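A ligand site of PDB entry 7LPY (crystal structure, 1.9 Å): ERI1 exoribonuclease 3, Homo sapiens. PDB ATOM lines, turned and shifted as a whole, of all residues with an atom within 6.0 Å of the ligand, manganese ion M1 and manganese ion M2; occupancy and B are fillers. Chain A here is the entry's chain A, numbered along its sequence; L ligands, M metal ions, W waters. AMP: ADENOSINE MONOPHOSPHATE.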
ATOM      1  N   ASP A  29       2.571 -25.906  -7.088  1.00  0.00           N
ATOM      2  CA  ASP A  29       2.869 -25.412  -8.427  1.00  0.00           C
ATOM      3  C   ASP A  29       1.828 -26.004  -9.362  1.00  0.00           C
ATOM      4  O   ASP A  29       1.898 -27.204  -9.646  1.00  0.00           O
ATOM      5  CB  ASP A  29       4.271 -25.822  -8.876  1.00  0.00           C
ATOM      6  CG  ASP A  29       4.672 -25.178 -10.188  1.00  0.00           C
ATOM      7  OD1 ASP A  29       4.945 -23.966 -10.168  1.00  0.00           O
ATOM      8  OD2 ASP A  29       4.717 -25.869 -11.233  1.00  0.00           O
ATOM      9  N   PHE A  30       0.863 -25.216  -9.823  1.00  0.00           N
ATOM     10  CA  PHE A  30      -0.121 -25.737 -10.752  1.00  0.00           C
ATOM     11  C   PHE A  30       0.499 -25.961 -12.123  1.00  0.00           C
ATOM     12  O   PHE A  30       1.435 -25.270 -12.529  1.00  0.00           O
ATOM     13  CB  PHE A  30      -1.278 -24.755 -10.930  1.00  0.00           C
ATOM     14  CG  PHE A  30      -2.086 -24.493  -9.689  1.00  0.00           C
ATOM     15  CD1 PHE A  30      -2.543 -25.546  -8.893  1.00  0.00           C
ATOM     16  CD2 PHE A  30      -2.372 -23.168  -9.301  1.00  0.00           C
ATOM     17  CE1 PHE A  30      -3.295 -25.299  -7.752  1.00  0.00           C
ATOM     18  CE2 PHE A  30      -3.124 -22.912  -8.163  1.00  0.00           C
ATOM     19  CZ  PHE A  30      -3.601 -23.992  -7.389  1.00  0.00           C
ATOM     20  N   GLU A  31      -0.040 -26.932 -12.866  1.00  0.00           N
ATOM     21  CA  GLU A  31       0.003 -26.842 -14.318  1.00  0.00           C
ATOM     22  C   GLU A  31      -1.417 -26.598 -14.818  1.00  0.00           C
ATOM     23  O   GLU A  31      -2.391 -26.986 -14.158  1.00  0.00           O
ATOM     24  CB  GLU A  31       0.580 -28.092 -14.988  1.00  0.00           C
ATOM     25  CG  GLU A  31       1.980 -28.474 -14.540  1.00  0.00           C
ATOM     26  CD  GLU A  31       3.013 -27.408 -14.795  1.00  0.00           C
ATOM     27  OE1 GLU A  31       2.909 -26.676 -15.811  1.00  0.00           O
ATOM     28  OE2 GLU A  31       3.969 -27.348 -13.990  1.00  0.00           O
ATOM     29  N   ALA A  32      -1.530 -25.941 -15.966  1.00  0.00           N
ATOM     30  CA  ALA A  32      -2.822 -25.540 -16.494  1.00  0.00           C
ATOM     31  C   ALA A  32      -2.851 -25.796 -17.990  1.00  0.00           C
ATOM     32  O   ALA A  32      -1.806 -25.890 -18.634  1.00  0.00           O
ATOM     33  CB  ALA A  32      -3.101 -24.038 -16.232  1.00  0.00           C
ATOM     34  N   THR A  33      -4.072 -25.901 -18.535  1.00  0.00           N
ATOM     35  CA  THR A  33      -4.239 -25.891 -19.983  1.00  0.00           C
ATOM     36  C   THR A  33      -3.576 -24.637 -20.563  1.00  0.00           C
ATOM     37  O   THR A  33      -3.515 -23.590 -19.920  1.00  0.00           O
ATOM     38  CB  THR A  33      -5.723 -25.894 -20.362  1.00  0.00           C
ATOM     39  OG1 THR A  33      -6.355 -24.758 -19.776  1.00  0.00           O
ATOM     40  CG2 THR A  33      -6.423 -27.161 -19.852  1.00  0.00           C
ATOM     41  N   CYS A  34      -3.078 -24.776 -21.789  1.00  0.00           N
ATOM     42  CA  CYS A  34      -2.376 -23.694 -22.460  1.00  0.00           C
ATOM     43  C   CYS A  34      -2.359 -23.986 -23.950  1.00  0.00           C
ATOM     44  O   CYS A  34      -2.778 -25.059 -24.399  1.00  0.00           O
ATOM     45  CB  CYS A  34      -0.958 -23.523 -21.903  1.00  0.00           C
ATOM     46  SG  CYS A  34      -0.009 -25.064 -21.859  1.00  0.00           S
ATOM     47  N   ASP A  35      -1.852 -23.014 -24.712  1.00  0.00           N
ATOM     48  CA  ASP A  35      -1.750 -23.124 -26.156  1.00  0.00           C
ATOM     49  C   ASP A  35      -0.891 -21.968 -26.647  1.00  0.00           C
ATOM     50  O   ASP A  35      -0.505 -21.081 -25.864  1.00  0.00           O
ATOM     51  CB  ASP A  35      -3.144 -23.132 -26.811  1.00  0.00           C
ATOM     52  CG  ASP A  35      -3.138 -23.751 -28.201  1.00  0.00           C
ATOM     53  OD1 ASP A  35      -2.060 -24.191 -28.669  1.00  0.00           O
ATOM     54  OD2 ASP A  35      -4.221 -23.837 -28.815  1.00  0.00           O
ATOM     55  N   LYS A  36      -0.625 -21.953 -27.943  1.00  0.00           N
ATOM     56  CA  LYS A  36       0.162 -20.893 -28.559  1.00  0.00           C
ATOM     57  C   LYS A  36      -0.643 -20.292 -29.695  1.00  0.00           C
ATOM     58  O   LYS A  36      -0.849 -20.961 -30.713  1.00  0.00           O
ATOM     59  CB  LYS A  36       1.483 -21.455 -29.089  1.00  0.00           C
ATOM     60  CG  LYS A  36       2.656 -20.627 -28.679  1.00  0.00           C
ATOM     61  CD  LYS A  36       2.938 -21.007 -27.250  1.00  0.00           C
ATOM     62  CE  LYS A  36       4.211 -20.413 -26.741  1.00  0.00           C
ATOM     63  NZ  LYS A  36       3.964 -19.529 -25.554  1.00  0.00           N
ATOM     64  N   GLN A  38      -1.959 -18.031 -26.131  1.00  0.00           N
ATOM     65  CA  GLN A  38      -2.481 -18.629 -24.907  1.00  0.00           C
ATOM     66  C   GLN A  38      -3.958 -18.961 -25.021  1.00  0.00           C
ATOM     67  O   GLN A  38      -4.735 -18.240 -25.665  1.00  0.00           O
ATOM     68  CB  GLN A  38      -2.238 -17.683 -23.731  1.00  0.00           C
ATOM     69  CG  GLN A  38      -2.442 -18.336 -22.377  1.00  0.00           C
ATOM     70  CD  GLN A  38      -1.656 -19.634 -22.243  1.00  0.00           C
ATOM     71  OE1 GLN A  38      -2.090 -20.676 -22.726  1.00  0.00           O
ATOM     72  NE2 GLN A  38      -0.495 -19.562 -21.610  1.00  0.00           N
ATOM     73  N   GLN A  42      -7.630 -20.327 -19.047  1.00  0.00           N
ATOM     74  CA  GLN A  42      -6.819 -21.442 -18.587  1.00  0.00           C
ATOM     75  C   GLN A  42      -7.539 -22.175 -17.465  1.00  0.00           C
ATOM     76  O   GLN A  42      -8.378 -21.602 -16.752  1.00  0.00           O
ATOM     77  CB  GLN A  42      -5.458 -20.986 -18.095  1.00  0.00           C
ATOM     78  CG  GLN A  42      -4.573 -20.372 -19.163  1.00  0.00           C
ATOM     79  CD  GLN A  42      -3.174 -20.132 -18.657  1.00  0.00           C
ATOM     80  OE1 GLN A  42      -2.867 -19.051 -18.172  1.00  0.00           O
ATOM     81  NE2 GLN A  42      -2.332 -21.146 -18.767  1.00  0.00           N
ATOM     82  N   ILE A  45      -4.867 -28.258 -14.447  1.00  0.00           N
ATOM     83  CA  ILE A  45      -4.889 -29.686 -14.759  1.00  0.00           C
ATOM     84  C   ILE A  45      -3.969 -30.512 -13.874  1.00  0.00           C
ATOM     85  O   ILE A  45      -3.997 -31.742 -13.965  1.00  0.00           O
ATOM     86  CB  ILE A  45      -4.538 -29.956 -16.249  1.00  0.00           C
ATOM     87  CG1 ILE A  45      -3.156 -29.395 -16.589  1.00  0.00           C
ATOM     88  CG2 ILE A  45      -5.601 -29.362 -17.163  1.00  0.00           C
ATOM     89  CD1 ILE A  45      -2.709 -29.675 -18.017  1.00  0.00           C
ATOM     90  N   PHE A  78       0.490 -28.369 -27.722  1.00  0.00           N
ATOM     91  CA  PHE A  78       1.458 -27.547 -26.992  1.00  0.00           C
ATOM     92  C   PHE A  78       1.412 -27.838 -25.501  1.00  0.00           C
ATOM     93  O   PHE A  78       2.452 -27.946 -24.841  1.00  0.00           O
ATOM     94  CB  PHE A  78       1.204 -26.061 -27.241  1.00  0.00           C
ATOM     95  CG  PHE A  78       2.104 -25.166 -26.435  1.00  0.00           C
ATOM     96  CD1 PHE A  78       3.372 -24.830 -26.912  1.00  0.00           C
ATOM     97  CD2 PHE A  78       1.710 -24.700 -25.200  1.00  0.00           C
ATOM     98  CE1 PHE A  78       4.215 -24.025 -26.157  1.00  0.00           C
ATOM     99  CE2 PHE A  78       2.542 -23.899 -24.432  1.00  0.00           C
ATOM    100  CZ  PHE A  78       3.801 -23.557 -24.924  1.00  0.00           C
ATOM    101  N   LEU A  82       4.556 -29.165 -23.445  1.00  0.00           N
ATOM    102  CA  LEU A  82       5.125 -28.359 -22.374  1.00  0.00           C
ATOM    103  C   LEU A  82       5.143 -29.129 -21.052  1.00  0.00           C
ATOM    104  O   LEU A  82       6.192 -29.255 -20.407  1.00  0.00           O
ATOM    105  CB  LEU A  82       4.339 -27.061 -22.216  1.00  0.00           C
ATOM    106  CG  LEU A  82       4.881 -26.118 -21.138  1.00  0.00           C
ATOM    107  CD1 LEU A  82       6.198 -25.478 -21.599  1.00  0.00           C
ATOM    108  CD2 LEU A  82       3.848 -25.045 -20.809  1.00  0.00           C
ATOM    109  N   THR A  83       3.992 -29.643 -20.628  1.00  0.00           N
ATOM    110  CA  THR A  83       3.859 -30.202 -19.289  1.00  0.00           C
ATOM    111  C   THR A  83       4.126 -31.689 -19.223  1.00  0.00           C
ATOM    112  O   THR A  83       4.367 -32.206 -18.117  1.00  0.00           O
ATOM    113  CB  THR A  83       2.456 -29.940 -18.747  1.00  0.00           C
ATOM    114  OG1 THR A  83       1.513 -30.660 -19.540  1.00  0.00           O
ATOM    115  CG2 THR A  83       2.128 -28.436 -18.790  1.00  0.00           C
ATOM    116  N   CYS A 124       6.457 -20.587  -6.794  1.00  0.00           N
ATOM    117  CA  CYS A 124       7.470 -19.903  -7.595  1.00  0.00           C
ATOM    118  C   CYS A 124       6.771 -18.793  -8.352  1.00  0.00           C
ATOM    119  O   CYS A 124       6.190 -19.021  -9.423  1.00  0.00           O
ATOM    120  CB  CYS A 124       8.168 -20.866  -8.563  1.00  0.00           C
ATOM    121  SG  CYS A 124       9.589 -20.094  -9.442  1.00  0.00           S
ATOM    122  N   TRP A 127       1.805 -16.124  -9.511  1.00  0.00           N
ATOM    123  CA  TRP A 127       0.729 -16.473 -10.449  1.00  0.00           C
ATOM    124  C   TRP A 127      -0.254 -17.498  -9.864  1.00  0.00           C
ATOM    125  O   TRP A 127      -1.478 -17.363 -10.032  1.00  0.00           O
ATOM    126  CB  TRP A 127       1.332 -17.000 -11.739  1.00  0.00           C
ATOM    127  CG  TRP A 127       0.333 -17.456 -12.783  1.00  0.00           C
ATOM    128  CD1 TRP A 127      -0.401 -16.646 -13.623  1.00  0.00           C
ATOM    129  CD2 TRP A 127      -0.022 -18.805 -13.116  1.00  0.00           C
ATOM    130  NE1 TRP A 127      -1.197 -17.415 -14.435  1.00  0.00           N
ATOM    131  CE2 TRP A 127      -0.979 -18.739 -14.145  1.00  0.00           C
ATOM    132  CE3 TRP A 127       0.381 -20.054 -12.635  1.00  0.00           C
ATOM    133  CZ2 TRP A 127      -1.537 -19.875 -14.712  1.00  0.00           C
ATOM    134  CZ3 TRP A 127      -0.188 -21.185 -13.194  1.00  0.00           C
ATOM    135  CH2 TRP A 127      -1.122 -21.090 -14.223  1.00  0.00           C
ATOM    136  N   ASP A 128       0.247 -18.546  -9.203  1.00  0.00           N
ATOM    137  CA  ASP A 128      -0.629 -19.659  -8.827  1.00  0.00           C
ATOM    138  C   ASP A 128      -1.805 -19.219  -7.962  1.00  0.00           C
ATOM    139  O   ASP A 128      -2.964 -19.526  -8.260  1.00  0.00           O
ATOM    140  CB  ASP A 128       0.187 -20.733  -8.102  1.00  0.00           C
ATOM    141  CG  ASP A 128       1.315 -21.246  -8.950  1.00  0.00           C
ATOM    142  OD1 ASP A 128       1.213 -22.383  -9.427  1.00  0.00           O
ATOM    143  OD2 ASP A 128       2.293 -20.490  -9.155  1.00  0.00           O
ATOM    144  N   HIS A 186       8.685 -28.280 -15.865  1.00  0.00           N
ATOM    145  CA  HIS A 186       7.285 -28.032 -16.215  1.00  0.00           C
ATOM    146  C   HIS A 186       6.366 -29.198 -15.873  1.00  0.00           C
ATOM    147  O   HIS A 186       5.236 -29.282 -16.392  1.00  0.00           O
ATOM    148  CB  HIS A 186       7.148 -27.648 -17.696  1.00  0.00           C
ATOM    149  CG  HIS A 186       8.076 -26.542 -18.099  1.00  0.00           C
ATOM    150  ND1 HIS A 186       7.817 -25.216 -17.808  1.00  0.00           N
ATOM    151  CD2 HIS A 186       9.268 -26.561 -18.726  1.00  0.00           C
ATOM    152  CE1 HIS A 186       8.811 -24.469 -18.246  1.00  0.00           C
ATOM    153  NE2 HIS A 186       9.698 -25.261 -18.813  1.00  0.00           N
ATOM    154  N   SER A 187       6.807 -30.106 -15.022  1.00  0.00           N
ATOM    155  CA  SER A 187       5.909 -30.992 -14.308  1.00  0.00           C
ATOM    156  C   SER A 187       5.559 -30.330 -12.979  1.00  0.00           C
ATOM    157  O   SER A 187       6.456 -29.828 -12.282  1.00  0.00           O
ATOM    158  CB  SER A 187       6.560 -32.366 -14.082  1.00  0.00           C
ATOM    159  OG  SER A 187       5.880 -33.085 -13.072  1.00  0.00           O
ATOM    160  N   GLY A 188       4.276 -30.303 -12.629  1.00  0.00           N
ATOM    161  CA  GLY A 188       3.903 -29.632 -11.391  1.00  0.00           C
ATOM    162  C   GLY A 188       4.590 -30.241 -10.179  1.00  0.00           C
ATOM    163  O   GLY A 188       5.218 -29.541  -9.377  1.00  0.00           O
ATOM    164  N   ASP A 191       8.322 -29.511 -10.312  1.00  0.00           N
ATOM    165  CA  ASP A 191       8.568 -28.126  -9.953  1.00  0.00           C
ATOM    166  C   ASP A 191       8.496 -27.957  -8.435  1.00  0.00           C
ATOM    167  O   ASP A 191       9.357 -27.294  -7.838  1.00  0.00           O
ATOM    168  CB  ASP A 191       7.575 -27.202 -10.676  1.00  0.00           C
ATOM    169  CG  ASP A 191       7.934 -27.001 -12.153  1.00  0.00           C
ATOM    170  OD1 ASP A 191       9.042 -27.389 -12.565  1.00  0.00           O
ATOM    171  OD2 ASP A 191       7.098 -26.437 -12.907  1.00  0.00           O
HETATM  172  P   AMP L   1       4.993 -22.823 -14.539  1.00  0.00           P
HETATM  173  O1P AMP L   1       4.730 -21.480 -13.886  1.00  0.00           O
HETATM  174  O2P AMP L   1       4.948 -23.969 -13.573  1.00  0.00           O
HETATM  175  O3P AMP L   1       6.202 -22.874 -15.454  1.00  0.00           O
HETATM  176  O5' AMP L   1       3.798 -23.022 -15.575  1.00  0.00           O
HETATM  177  C5' AMP L   1       2.435 -22.951 -15.169  1.00  0.00           C
HETATM  178  C4' AMP L   1       1.495 -22.932 -16.362  1.00  0.00           C
HETATM  179  O4' AMP L   1       1.684 -21.708 -17.118  1.00  0.00           O
HETATM  180  C3' AMP L   1       1.688 -24.048 -17.391  1.00  0.00           C
HETATM  181  O3' AMP L   1       1.071 -25.278 -17.003  1.00  0.00           O
HETATM  182  C2' AMP L   1       1.086 -23.426 -18.648  1.00  0.00           C
HETATM  183  O2' AMP L   1      -0.343 -23.468 -18.598  1.00  0.00           O
HETATM  184  C1' AMP L   1       1.535 -21.967 -18.498  1.00  0.00           C
HETATM  185  N9  AMP L   1       2.843 -21.760 -19.148  1.00  0.00           N
HETATM  186  C8  AMP L   1       4.052 -21.941 -18.562  1.00  0.00           C
HETATM  187  N7  AMP L   1       5.057 -21.709 -19.459  1.00  0.00           N
HETATM  188  C5  AMP L   1       4.469 -21.378 -20.629  1.00  0.00           C
HETATM  189  C6  AMP L   1       4.936 -21.025 -21.992  1.00  0.00           C
HETATM  190  N6  AMP L   1       6.262 -20.967 -22.278  1.00  0.00           N
HETATM  191  N1  AMP L   1       4.011 -20.772 -22.924  1.00  0.00           N
HETATM  192  C2  AMP L   1       2.695 -20.842 -22.665  1.00  0.00           C
HETATM  193  N3  AMP L   1       2.205 -21.149 -21.462  1.00  0.00           N
HETATM  194  C4  AMP L   1       3.018 -21.431 -20.424  1.00  0.00           C
HETATM  195 MN    MN M   1       5.280 -25.821 -13.236  1.00  0.00          MN
HETATM  196 MN    MN M   2       4.737 -22.517 -11.807  1.00  0.00          MN
HETATM  197  O   HOH W   1       0.119 -18.959 -17.946  1.00  0.00           O
HETATM  198  O   HOH W   2       8.069 -20.836 -15.963  1.00  0.00           O
HETATM  199  O   HOH W   3       7.088 -22.469 -11.788  1.00  0.00           O
HETATM  200  O   HOH W   4       4.225 -20.754 -10.469  1.00  0.00           O
HETATM  201  O   HOH W   5       5.520 -25.704 -15.147  1.00  0.00           O
HETATM  202  O   HOH W   6       2.559 -22.790 -11.761  1.00  0.00           O
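Residues that only touch the ligand: Phe 78 (3.4 Å), Phe 30 (3.7 Å), His 186 (3.7 Å), Leu 82 (3.7 Å), Trp 127 (3.7 Å) and Thr 83 (3.8 Å).
Within 4 Å of the ligand: Asp 29, Phe 30, Glu 31, Ala 32, Thr 33, Cys 34, Lys 36, Gln 38, Gln 42, Phe 78, Leu 82, Thr 83, Trp 127, His 186 and Asp 191.
Phe 30 touches manganese ion M1 (O to MN, 3.9 Å).
Four residues have an atom within 4 Å of manganese ion M1: Asp 29, Phe 30, Glu 31 and Asp 191.
The nearest printed residue that does not touch manganese ion M1 is His 186 (4.2 Å).
OD1 of Asp 191 sits at hydrogen-bond distance from N of His 186 (3.4 Å).
The side-chain carboxylate of Glu 31 sits close to the backbone NH of Gly 188, 3.3 Å away.
The backbone NH of Ile 45 lies within hydrogen-bond range of the backbone carbonyl oxygen of Glu 31 (2.8 Å).
The backbone carbonyl oxygen (O) of Ala 32 sits at hydrogen-bond distance from the side-chain sulfur (SG) of Cys 34 (3.8 Å).
The backbone carbonyl oxygen of Thr 33 is in hydrogen-bond range of the side-chain amide nitrogen of Gln 42.
N of Asp 35 lies within hydrogen-bond range of OE1 of Gln 38, 3.1 Å away.
The backbone NH (N) of Phe 30 is in hydrogen-bond range of the side-chain carboxylate (OD1) of Asp 128, 2.9 Å away.
Manganese ion M1 is bound by O2P of the ligand (1.9 Å), water W5 (1.9 Å), OD2 of Asp 191 (1.9 Å), OD2 of Asp 29 (2.1 Å) and OE2 of Glu 31 (2.1 Å).
Water W5 lies within hydrogen-bond range of OE1 of Glu 31 (2.9 Å) and O3P of the ligand (2.9 Å).
Water W6 bridges OD1 of Asp 128 (2.7 Å) and O of Phe 30 (2.8 Å).
Water W1 lies within hydrogen-bond range of the side-chain amide oxygen of Gln 42 (3.0 Å) and an oxygen (O4') of the ligand (3.3 Å).
The backbone NH (N) of Ala 32 sits at hydrogen-bond distance from an oxygen (O3') of the ligand (2.9 Å).
O2' of the ligand is in hydrogen-bond range of O of Ala 32.
The side-chain amino group (NZ) of Lys 36 sits at hydrogen-bond distance from a nitrogen (N1) of the ligand (2.9 Å).
The side-chain amide nitrogen (NE2) of Gln 42 is in hydrogen-bond range of an oxygen (O2') of the ligand, 3.1 Å away.
The side-chain amide nitrogen of Gln 38 lies within hydrogen-bond range of a nitrogen (N3) of the ligand (3.1 Å).
SG of Cys 34 lies close to O2' of the ligand (3.6 Å).
O2' of the ligand lies within hydrogen-bond range of O of Thr 33 (3.4 Å).
Manganese ion M2 is bound by water W6 (2.2 Å), OD1 of Asp 29 (2.2 Å), water W4 (2.3 Å), O2P of the ligand (2.3 Å), O1P of the ligand (2.3 Å) and water W3 (2.4 Å).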
